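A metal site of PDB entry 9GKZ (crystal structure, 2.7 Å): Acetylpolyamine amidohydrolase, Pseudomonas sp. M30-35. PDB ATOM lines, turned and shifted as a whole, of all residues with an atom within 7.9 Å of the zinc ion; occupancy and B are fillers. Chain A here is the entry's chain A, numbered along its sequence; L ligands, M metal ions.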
ATOM      1  N   PRO A 167     -19.114 -15.698 -23.593  1.00  0.00           N
ATOM      2  CA  PRO A 167     -19.335 -14.351 -24.126  1.00  0.00           C
ATOM      3  C   PRO A 167     -20.283 -14.410 -25.318  1.00  0.00           C
ATOM      4  O   PRO A 167     -20.663 -15.482 -25.788  1.00  0.00           O
ATOM      5  CB  PRO A 167     -17.928 -13.888 -24.531  1.00  0.00           C
ATOM      6  CG  PRO A 167     -17.234 -15.161 -24.902  1.00  0.00           C
ATOM      7  CD  PRO A 167     -17.767 -16.210 -23.921  1.00  0.00           C
ATOM      8  N   HIS A 169     -20.498 -11.353 -28.008  1.00  0.00           N
ATOM      9  CA  HIS A 169     -20.432 -10.289 -29.018  1.00  0.00           C
ATOM     10  C   HIS A 169     -19.967 -10.748 -30.407  1.00  0.00           C
ATOM     11  O   HIS A 169     -20.111  -9.973 -31.358  1.00  0.00           O
ATOM     12  CB  HIS A 169     -19.551  -9.123 -28.514  1.00  0.00           C
ATOM     13  CG  HIS A 169     -18.069  -9.365 -28.631  1.00  0.00           C
ATOM     14  ND1 HIS A 169     -17.173  -8.324 -28.748  1.00  0.00           N
ATOM     15  CD2 HIS A 169     -17.333 -10.498 -28.609  1.00  0.00           C
ATOM     16  CE1 HIS A 169     -15.944  -8.810 -28.816  1.00  0.00           C
ATOM     17  NE2 HIS A 169     -16.012 -10.122 -28.728  1.00  0.00           N
ATOM     18  N   HIS A 170     -19.441 -11.978 -30.553  1.00  0.00           N
ATOM     19  CA  HIS A 170     -19.171 -12.508 -31.886  1.00  0.00           C
ATOM     20  C   HIS A 170     -20.360 -13.230 -32.510  1.00  0.00           C
ATOM     21  O   HIS A 170     -20.291 -13.630 -33.676  1.00  0.00           O
ATOM     22  CB  HIS A 170     -17.972 -13.484 -31.890  1.00  0.00           C
ATOM     23  CG  HIS A 170     -16.674 -12.869 -31.466  1.00  0.00           C
ATOM     24  ND1 HIS A 170     -16.128 -11.757 -32.067  1.00  0.00           N
ATOM     25  CD2 HIS A 170     -15.801 -13.232 -30.484  1.00  0.00           C
ATOM     26  CE1 HIS A 170     -14.998 -11.447 -31.472  1.00  0.00           C
ATOM     27  NE2 HIS A 170     -14.769 -12.323 -30.509  1.00  0.00           N
ATOM     28  N   GLY A 178     -16.389 -17.802 -32.336  1.00  0.00           N
ATOM     29  CA  GLY A 178     -15.503 -17.213 -31.349  1.00  0.00           C
ATOM     30  C   GLY A 178     -15.961 -17.366 -29.908  1.00  0.00           C
ATOM     31  O   GLY A 178     -15.999 -16.377 -29.173  1.00  0.00           O
ATOM     32  N   CYS A 180     -18.857 -17.598 -28.903  1.00  0.00           N
ATOM     33  CA  CYS A 180     -20.097 -16.860 -28.716  1.00  0.00           C
ATOM     34  C   CYS A 180     -21.245 -17.624 -29.366  1.00  0.00           C
ATOM     35  O   CYS A 180     -21.198 -17.929 -30.554  1.00  0.00           O
ATOM     36  CB  CYS A 180     -19.994 -15.451 -29.284  1.00  0.00           C
ATOM     37  SG  CYS A 180     -18.793 -14.433 -28.415  1.00  0.00           S
ATOM     38  N   ASP A 204     -18.264  -1.353 -27.139  1.00  0.00           N
ATOM     39  CA  ASP A 204     -17.616  -2.663 -27.110  1.00  0.00           C
ATOM     40  C   ASP A 204     -16.112  -2.455 -26.928  1.00  0.00           C
ATOM     41  O   ASP A 204     -15.398  -2.200 -27.900  1.00  0.00           O
ATOM     42  CB  ASP A 204     -17.917  -3.391 -28.404  1.00  0.00           C
ATOM     43  CG  ASP A 204     -17.475  -4.814 -28.377  1.00  0.00           C
ATOM     44  OD1 ASP A 204     -16.351  -5.077 -27.876  1.00  0.00           O
ATOM     45  OD2 ASP A 204     -18.236  -5.665 -28.868  1.00  0.00           O
ATOM     46  N   VAL A 205     -15.648  -2.593 -25.691  1.00  0.00           N
ATOM     47  CA  VAL A 205     -14.256  -2.358 -25.342  1.00  0.00           C
ATOM     48  C   VAL A 205     -13.423  -3.631 -25.418  1.00  0.00           C
ATOM     49  O   VAL A 205     -12.212  -3.590 -25.124  1.00  0.00           O
ATOM     50  CB  VAL A 205     -14.157  -1.728 -23.931  1.00  0.00           C
ATOM     51  CG1 VAL A 205     -14.969  -0.453 -23.861  1.00  0.00           C
ATOM     52  CG2 VAL A 205     -14.639  -2.711 -22.898  1.00  0.00           C
ATOM     53  N   ASP A 206     -14.021  -4.757 -25.800  1.00  0.00           N
ATOM     54  CA  ASP A 206     -13.280  -5.988 -26.035  1.00  0.00           C
ATOM     55  C   ASP A 206     -12.161  -5.783 -27.061  1.00  0.00           C
ATOM     56  O   ASP A 206     -12.268  -4.967 -27.992  1.00  0.00           O
ATOM     57  CB  ASP A 206     -14.239  -7.080 -26.509  1.00  0.00           C
ATOM     58  CG  ASP A 206     -13.686  -8.470 -26.321  1.00  0.00           C
ATOM     59  OD1 ASP A 206     -12.942  -8.970 -27.195  1.00  0.00           O
ATOM     60  OD2 ASP A 206     -13.977  -9.060 -25.275  1.00  0.00           O
ATOM     61  N   TYR A 207     -11.079  -6.550 -26.916  1.00  0.00           N
ATOM     62  CA  TYR A 207      -9.989  -6.455 -27.889  1.00  0.00           C
ATOM     63  C   TYR A 207     -10.449  -6.797 -29.308  1.00  0.00           C
ATOM     64  O   TYR A 207      -9.848  -6.326 -30.276  1.00  0.00           O
ATOM     65  CB  TYR A 207      -8.808  -7.351 -27.491  1.00  0.00           C
ATOM     66  CG  TYR A 207      -7.774  -7.451 -28.566  1.00  0.00           C
ATOM     67  CD1 TYR A 207      -7.121  -6.319 -29.037  1.00  0.00           C
ATOM     68  CD2 TYR A 207      -7.475  -8.662 -29.157  1.00  0.00           C
ATOM     69  CE1 TYR A 207      -6.181  -6.409 -30.054  1.00  0.00           C
ATOM     70  CE2 TYR A 207      -6.544  -8.753 -30.185  1.00  0.00           C
ATOM     71  CZ  TYR A 207      -5.895  -7.619 -30.626  1.00  0.00           C
ATOM     72  OH  TYR A 207      -4.951  -7.722 -31.644  1.00  0.00           O
ATOM     73  N   HIS A 208     -11.527  -7.564 -29.443  1.00  0.00           N
ATOM     74  CA  HIS A 208     -11.950  -8.086 -30.734  1.00  0.00           C
ATOM     75  C   HIS A 208     -13.201  -7.358 -31.201  1.00  0.00           C
ATOM     76  O   HIS A 208     -13.963  -6.810 -30.390  1.00  0.00           O
ATOM     77  CB  HIS A 208     -12.237  -9.583 -30.656  1.00  0.00           C
ATOM     78  CG  HIS A 208     -11.042 -10.429 -30.363  1.00  0.00           C
ATOM     79  ND1 HIS A 208     -10.645 -10.727 -29.083  1.00  0.00           N
ATOM     80  CD2 HIS A 208     -10.169 -11.043 -31.177  1.00  0.00           C
ATOM     81  CE1 HIS A 208      -9.568 -11.476 -29.122  1.00  0.00           C
ATOM     82  NE2 HIS A 208      -9.261 -11.701 -30.379  1.00  0.00           N
ATOM     83  N   HIS A 209     -13.419  -7.347 -32.515  1.00  0.00           N
ATOM     84  CA  HIS A 209     -14.630  -6.730 -33.050  1.00  0.00           C
ATOM     85  C   HIS A 209     -15.868  -7.463 -32.560  1.00  0.00           C
ATOM     86  O   HIS A 209     -15.892  -8.691 -32.470  1.00  0.00           O
ATOM     87  CB  HIS A 209     -14.620  -6.711 -34.586  1.00  0.00           C
ATOM     88  CG  HIS A 209     -15.719  -5.879 -35.177  1.00  0.00           C
ATOM     89  ND1 HIS A 209     -16.682  -6.394 -36.028  1.00  0.00           N
ATOM     90  CD2 HIS A 209     -16.014  -4.564 -35.034  1.00  0.00           C
ATOM     91  CE1 HIS A 209     -17.511  -5.436 -36.393  1.00  0.00           C
ATOM     92  NE2 HIS A 209     -17.128  -4.319 -35.807  1.00  0.00           N
ATOM     93  N   PHE A 236      -8.412 -11.212 -35.759  1.00  0.00           N
ATOM     94  CA  PHE A 236      -9.749 -11.797 -35.647  1.00  0.00           C
ATOM     95  C   PHE A 236     -10.775 -10.712 -35.325  1.00  0.00           C
ATOM     96  O   PHE A 236     -10.532  -9.879 -34.434  1.00  0.00           O
ATOM     97  CB  PHE A 236      -9.773 -12.866 -34.552  1.00  0.00           C
ATOM     98  CG  PHE A 236     -11.000 -13.710 -34.577  1.00  0.00           C
ATOM     99  CD1 PHE A 236     -11.088 -14.799 -35.410  1.00  0.00           C
ATOM    100  CD2 PHE A 236     -12.085 -13.407 -33.772  1.00  0.00           C
ATOM    101  CE1 PHE A 236     -12.231 -15.573 -35.444  1.00  0.00           C
ATOM    102  CE2 PHE A 236     -13.220 -14.181 -33.793  1.00  0.00           C
ATOM    103  CZ  PHE A 236     -13.294 -15.263 -34.638  1.00  0.00           C
ATOM    104  N   GLY A 293     -14.935  -6.658 -22.431  1.00  0.00           N
ATOM    105  CA  GLY A 293     -13.822  -7.602 -22.507  1.00  0.00           C
ATOM    106  C   GLY A 293     -12.546  -6.923 -22.056  1.00  0.00           C
ATOM    107  O   GLY A 293     -12.324  -5.746 -22.339  1.00  0.00           O
ATOM    108  N   VAL A 294     -11.708  -7.667 -21.311  1.00  0.00           N
ATOM    109  CA  VAL A 294     -10.453  -7.075 -20.835  1.00  0.00           C
ATOM    110  C   VAL A 294      -9.267  -7.832 -21.393  1.00  0.00           C
ATOM    111  O   VAL A 294      -8.207  -7.901 -20.771  1.00  0.00           O
ATOM    112  CB  VAL A 294     -10.390  -7.008 -19.292  1.00  0.00           C
ATOM    113  CG1 VAL A 294     -11.300  -5.876 -18.797  1.00  0.00           C
ATOM    114  CG2 VAL A 294     -10.736  -8.366 -18.639  1.00  0.00           C
ATOM    115  N   ASP A 295      -9.455  -8.401 -22.606  1.00  0.00           N
ATOM    116  CA  ASP A 295      -8.369  -9.024 -23.346  1.00  0.00           C
ATOM    117  C   ASP A 295      -7.538  -8.008 -24.145  1.00  0.00           C
ATOM    118  O   ASP A 295      -6.776  -8.403 -25.018  1.00  0.00           O
ATOM    119  CB  ASP A 295      -8.894 -10.145 -24.268  1.00  0.00           C
ATOM    120  CG  ASP A 295     -10.021  -9.702 -25.178  1.00  0.00           C
ATOM    121  OD1 ASP A 295     -10.527  -8.571 -25.034  1.00  0.00           O
ATOM    122  OD2 ASP A 295     -10.424 -10.513 -26.052  1.00  0.00           O
ATOM    123  N   THR A 296      -7.703  -6.711 -23.866  1.00  0.00           N
ATOM    124  CA  THR A 296      -6.790  -5.671 -24.305  1.00  0.00           C
ATOM    125  C   THR A 296      -5.516  -5.603 -23.469  1.00  0.00           C
ATOM    126  O   THR A 296      -4.572  -4.906 -23.870  1.00  0.00           O
ATOM    127  CB  THR A 296      -7.462  -4.282 -24.265  1.00  0.00           C
ATOM    128  OG1 THR A 296      -8.200  -4.163 -23.047  1.00  0.00           O
ATOM    129  CG2 THR A 296      -8.379  -4.052 -25.435  1.00  0.00           C
ATOM    130  N   ASP A 300      -2.317 -10.267 -21.594  1.00  0.00           N
ATOM    131  CA  ASP A 300      -3.237 -11.258 -22.144  1.00  0.00           C
ATOM    132  C   ASP A 300      -2.584 -11.928 -23.337  1.00  0.00           C
ATOM    133  O   ASP A 300      -1.978 -11.239 -24.168  1.00  0.00           O
ATOM    134  CB  ASP A 300      -4.543 -10.589 -22.545  1.00  0.00           C
ATOM    135  CG  ASP A 300      -5.705 -11.565 -22.654  1.00  0.00           C
ATOM    136  OD1 ASP A 300      -5.713 -12.379 -23.615  1.00  0.00           O
ATOM    137  OD2 ASP A 300      -6.609 -11.486 -21.787  1.00  0.00           O
ATOM    138  N   ILE A 302      -3.807 -13.397 -26.031  1.00  0.00           N
ATOM    139  CA  ILE A 302      -4.402 -13.115 -27.331  1.00  0.00           C
ATOM    140  C   ILE A 302      -4.341 -11.630 -27.683  1.00  0.00           C
ATOM    141  O   ILE A 302      -4.614 -11.260 -28.834  1.00  0.00           O
ATOM    142  CB  ILE A 302      -5.845 -13.629 -27.344  1.00  0.00           C
ATOM    143  CG1 ILE A 302      -6.144 -14.280 -28.693  1.00  0.00           C
ATOM    144  CG2 ILE A 302      -6.826 -12.512 -26.980  1.00  0.00           C
ATOM    145  CD1 ILE A 302      -5.431 -15.634 -28.936  1.00  0.00           C
ATOM    146  N   GLU A 331     -17.465  -9.867 -21.707  1.00  0.00           N
ATOM    147  CA  GLU A 331     -17.073 -10.535 -22.936  1.00  0.00           C
ATOM    148  C   GLU A 331     -15.769 -11.300 -22.716  1.00  0.00           C
ATOM    149  O   GLU A 331     -15.686 -12.123 -21.802  1.00  0.00           O
ATOM    150  CB  GLU A 331     -16.929  -9.535 -24.092  1.00  0.00           C
ATOM    151  CG  GLU A 331     -18.137  -8.689 -24.366  1.00  0.00           C
ATOM    152  CD  GLU A 331     -19.238  -9.429 -25.114  1.00  0.00           C
ATOM    153  OE1 GLU A 331     -18.996 -10.595 -25.528  1.00  0.00           O
ATOM    154  OE2 GLU A 331     -20.346  -8.841 -25.298  1.00  0.00           O
ATOM    155  N   GLY A 332     -14.733 -10.978 -23.501  1.00  0.00           N
ATOM    156  CA  GLY A 332     -13.513 -11.774 -23.542  1.00  0.00           C
ATOM    157  C   GLY A 332     -12.480 -11.456 -22.463  1.00  0.00           C
ATOM    158  O   GLY A 332     -12.556 -10.501 -21.695  1.00  0.00           O
ATOM    159  N   GLY A 333     -11.473 -12.319 -22.418  1.00  0.00           N
ATOM    160  CA  GLY A 333     -10.355 -12.142 -21.507  1.00  0.00           C
ATOM    161  C   GLY A 333      -9.827 -13.475 -21.042  1.00  0.00           C
ATOM    162  O   GLY A 333     -10.574 -14.250 -20.440  1.00  0.00           O
ATOM    163  N   TYR A 334      -8.560 -13.764 -21.321  1.00  0.00           N
ATOM    164  CA  TYR A 334      -7.946 -14.987 -20.819  1.00  0.00           C
ATOM    165  C   TYR A 334      -7.854 -14.953 -19.294  1.00  0.00           C
ATOM    166  O   TYR A 334      -7.591 -13.911 -18.699  1.00  0.00           O
ATOM    167  CB  TYR A 334      -6.553 -15.183 -21.432  1.00  0.00           C
ATOM    168  CG  TYR A 334      -6.019 -16.609 -21.411  1.00  0.00           C
ATOM    169  CD1 TYR A 334      -5.648 -17.223 -20.214  1.00  0.00           C
ATOM    170  CD2 TYR A 334      -5.917 -17.352 -22.586  1.00  0.00           C
ATOM    171  CE1 TYR A 334      -5.173 -18.533 -20.199  1.00  0.00           C
ATOM    172  CE2 TYR A 334      -5.449 -18.657 -22.575  1.00  0.00           C
ATOM    173  CZ  TYR A 334      -5.073 -19.247 -21.375  1.00  0.00           C
ATOM    174  OH  TYR A 334      -4.604 -20.544 -21.358  1.00  0.00           O
HETATM  175 CL1  LIG L   1     -13.886 -12.753 -27.188  1.00  0.00          CL
HETATM  176 ZN    ZN M   1     -12.103 -10.772 -27.325  1.00  0.00          ZN
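The zinc ion is bound by OD1 of Asp 206 (2.0 Å), OD2 of Asp 295 (2.1 Å), ND1 of His 208 (2.3 Å) and CL1 of the ligand (2.7 Å).
The side-chain carboxylate (OD2) of Asp 206 is in hydrogen-bond range of the backbone NH (N) of Gly 332 (2.7 Å).
The backbone NH of Asp 206 sits at hydrogen-bond distance from the side-chain carboxylate of Asp 204, 3.1 Å away.
N of Tyr 207 lies within hydrogen-bond range of OD1 of Asp 295 (2.8 Å).
The nearest printed residue that does not touch the zinc ion is Gly 332 (4.2 Å).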
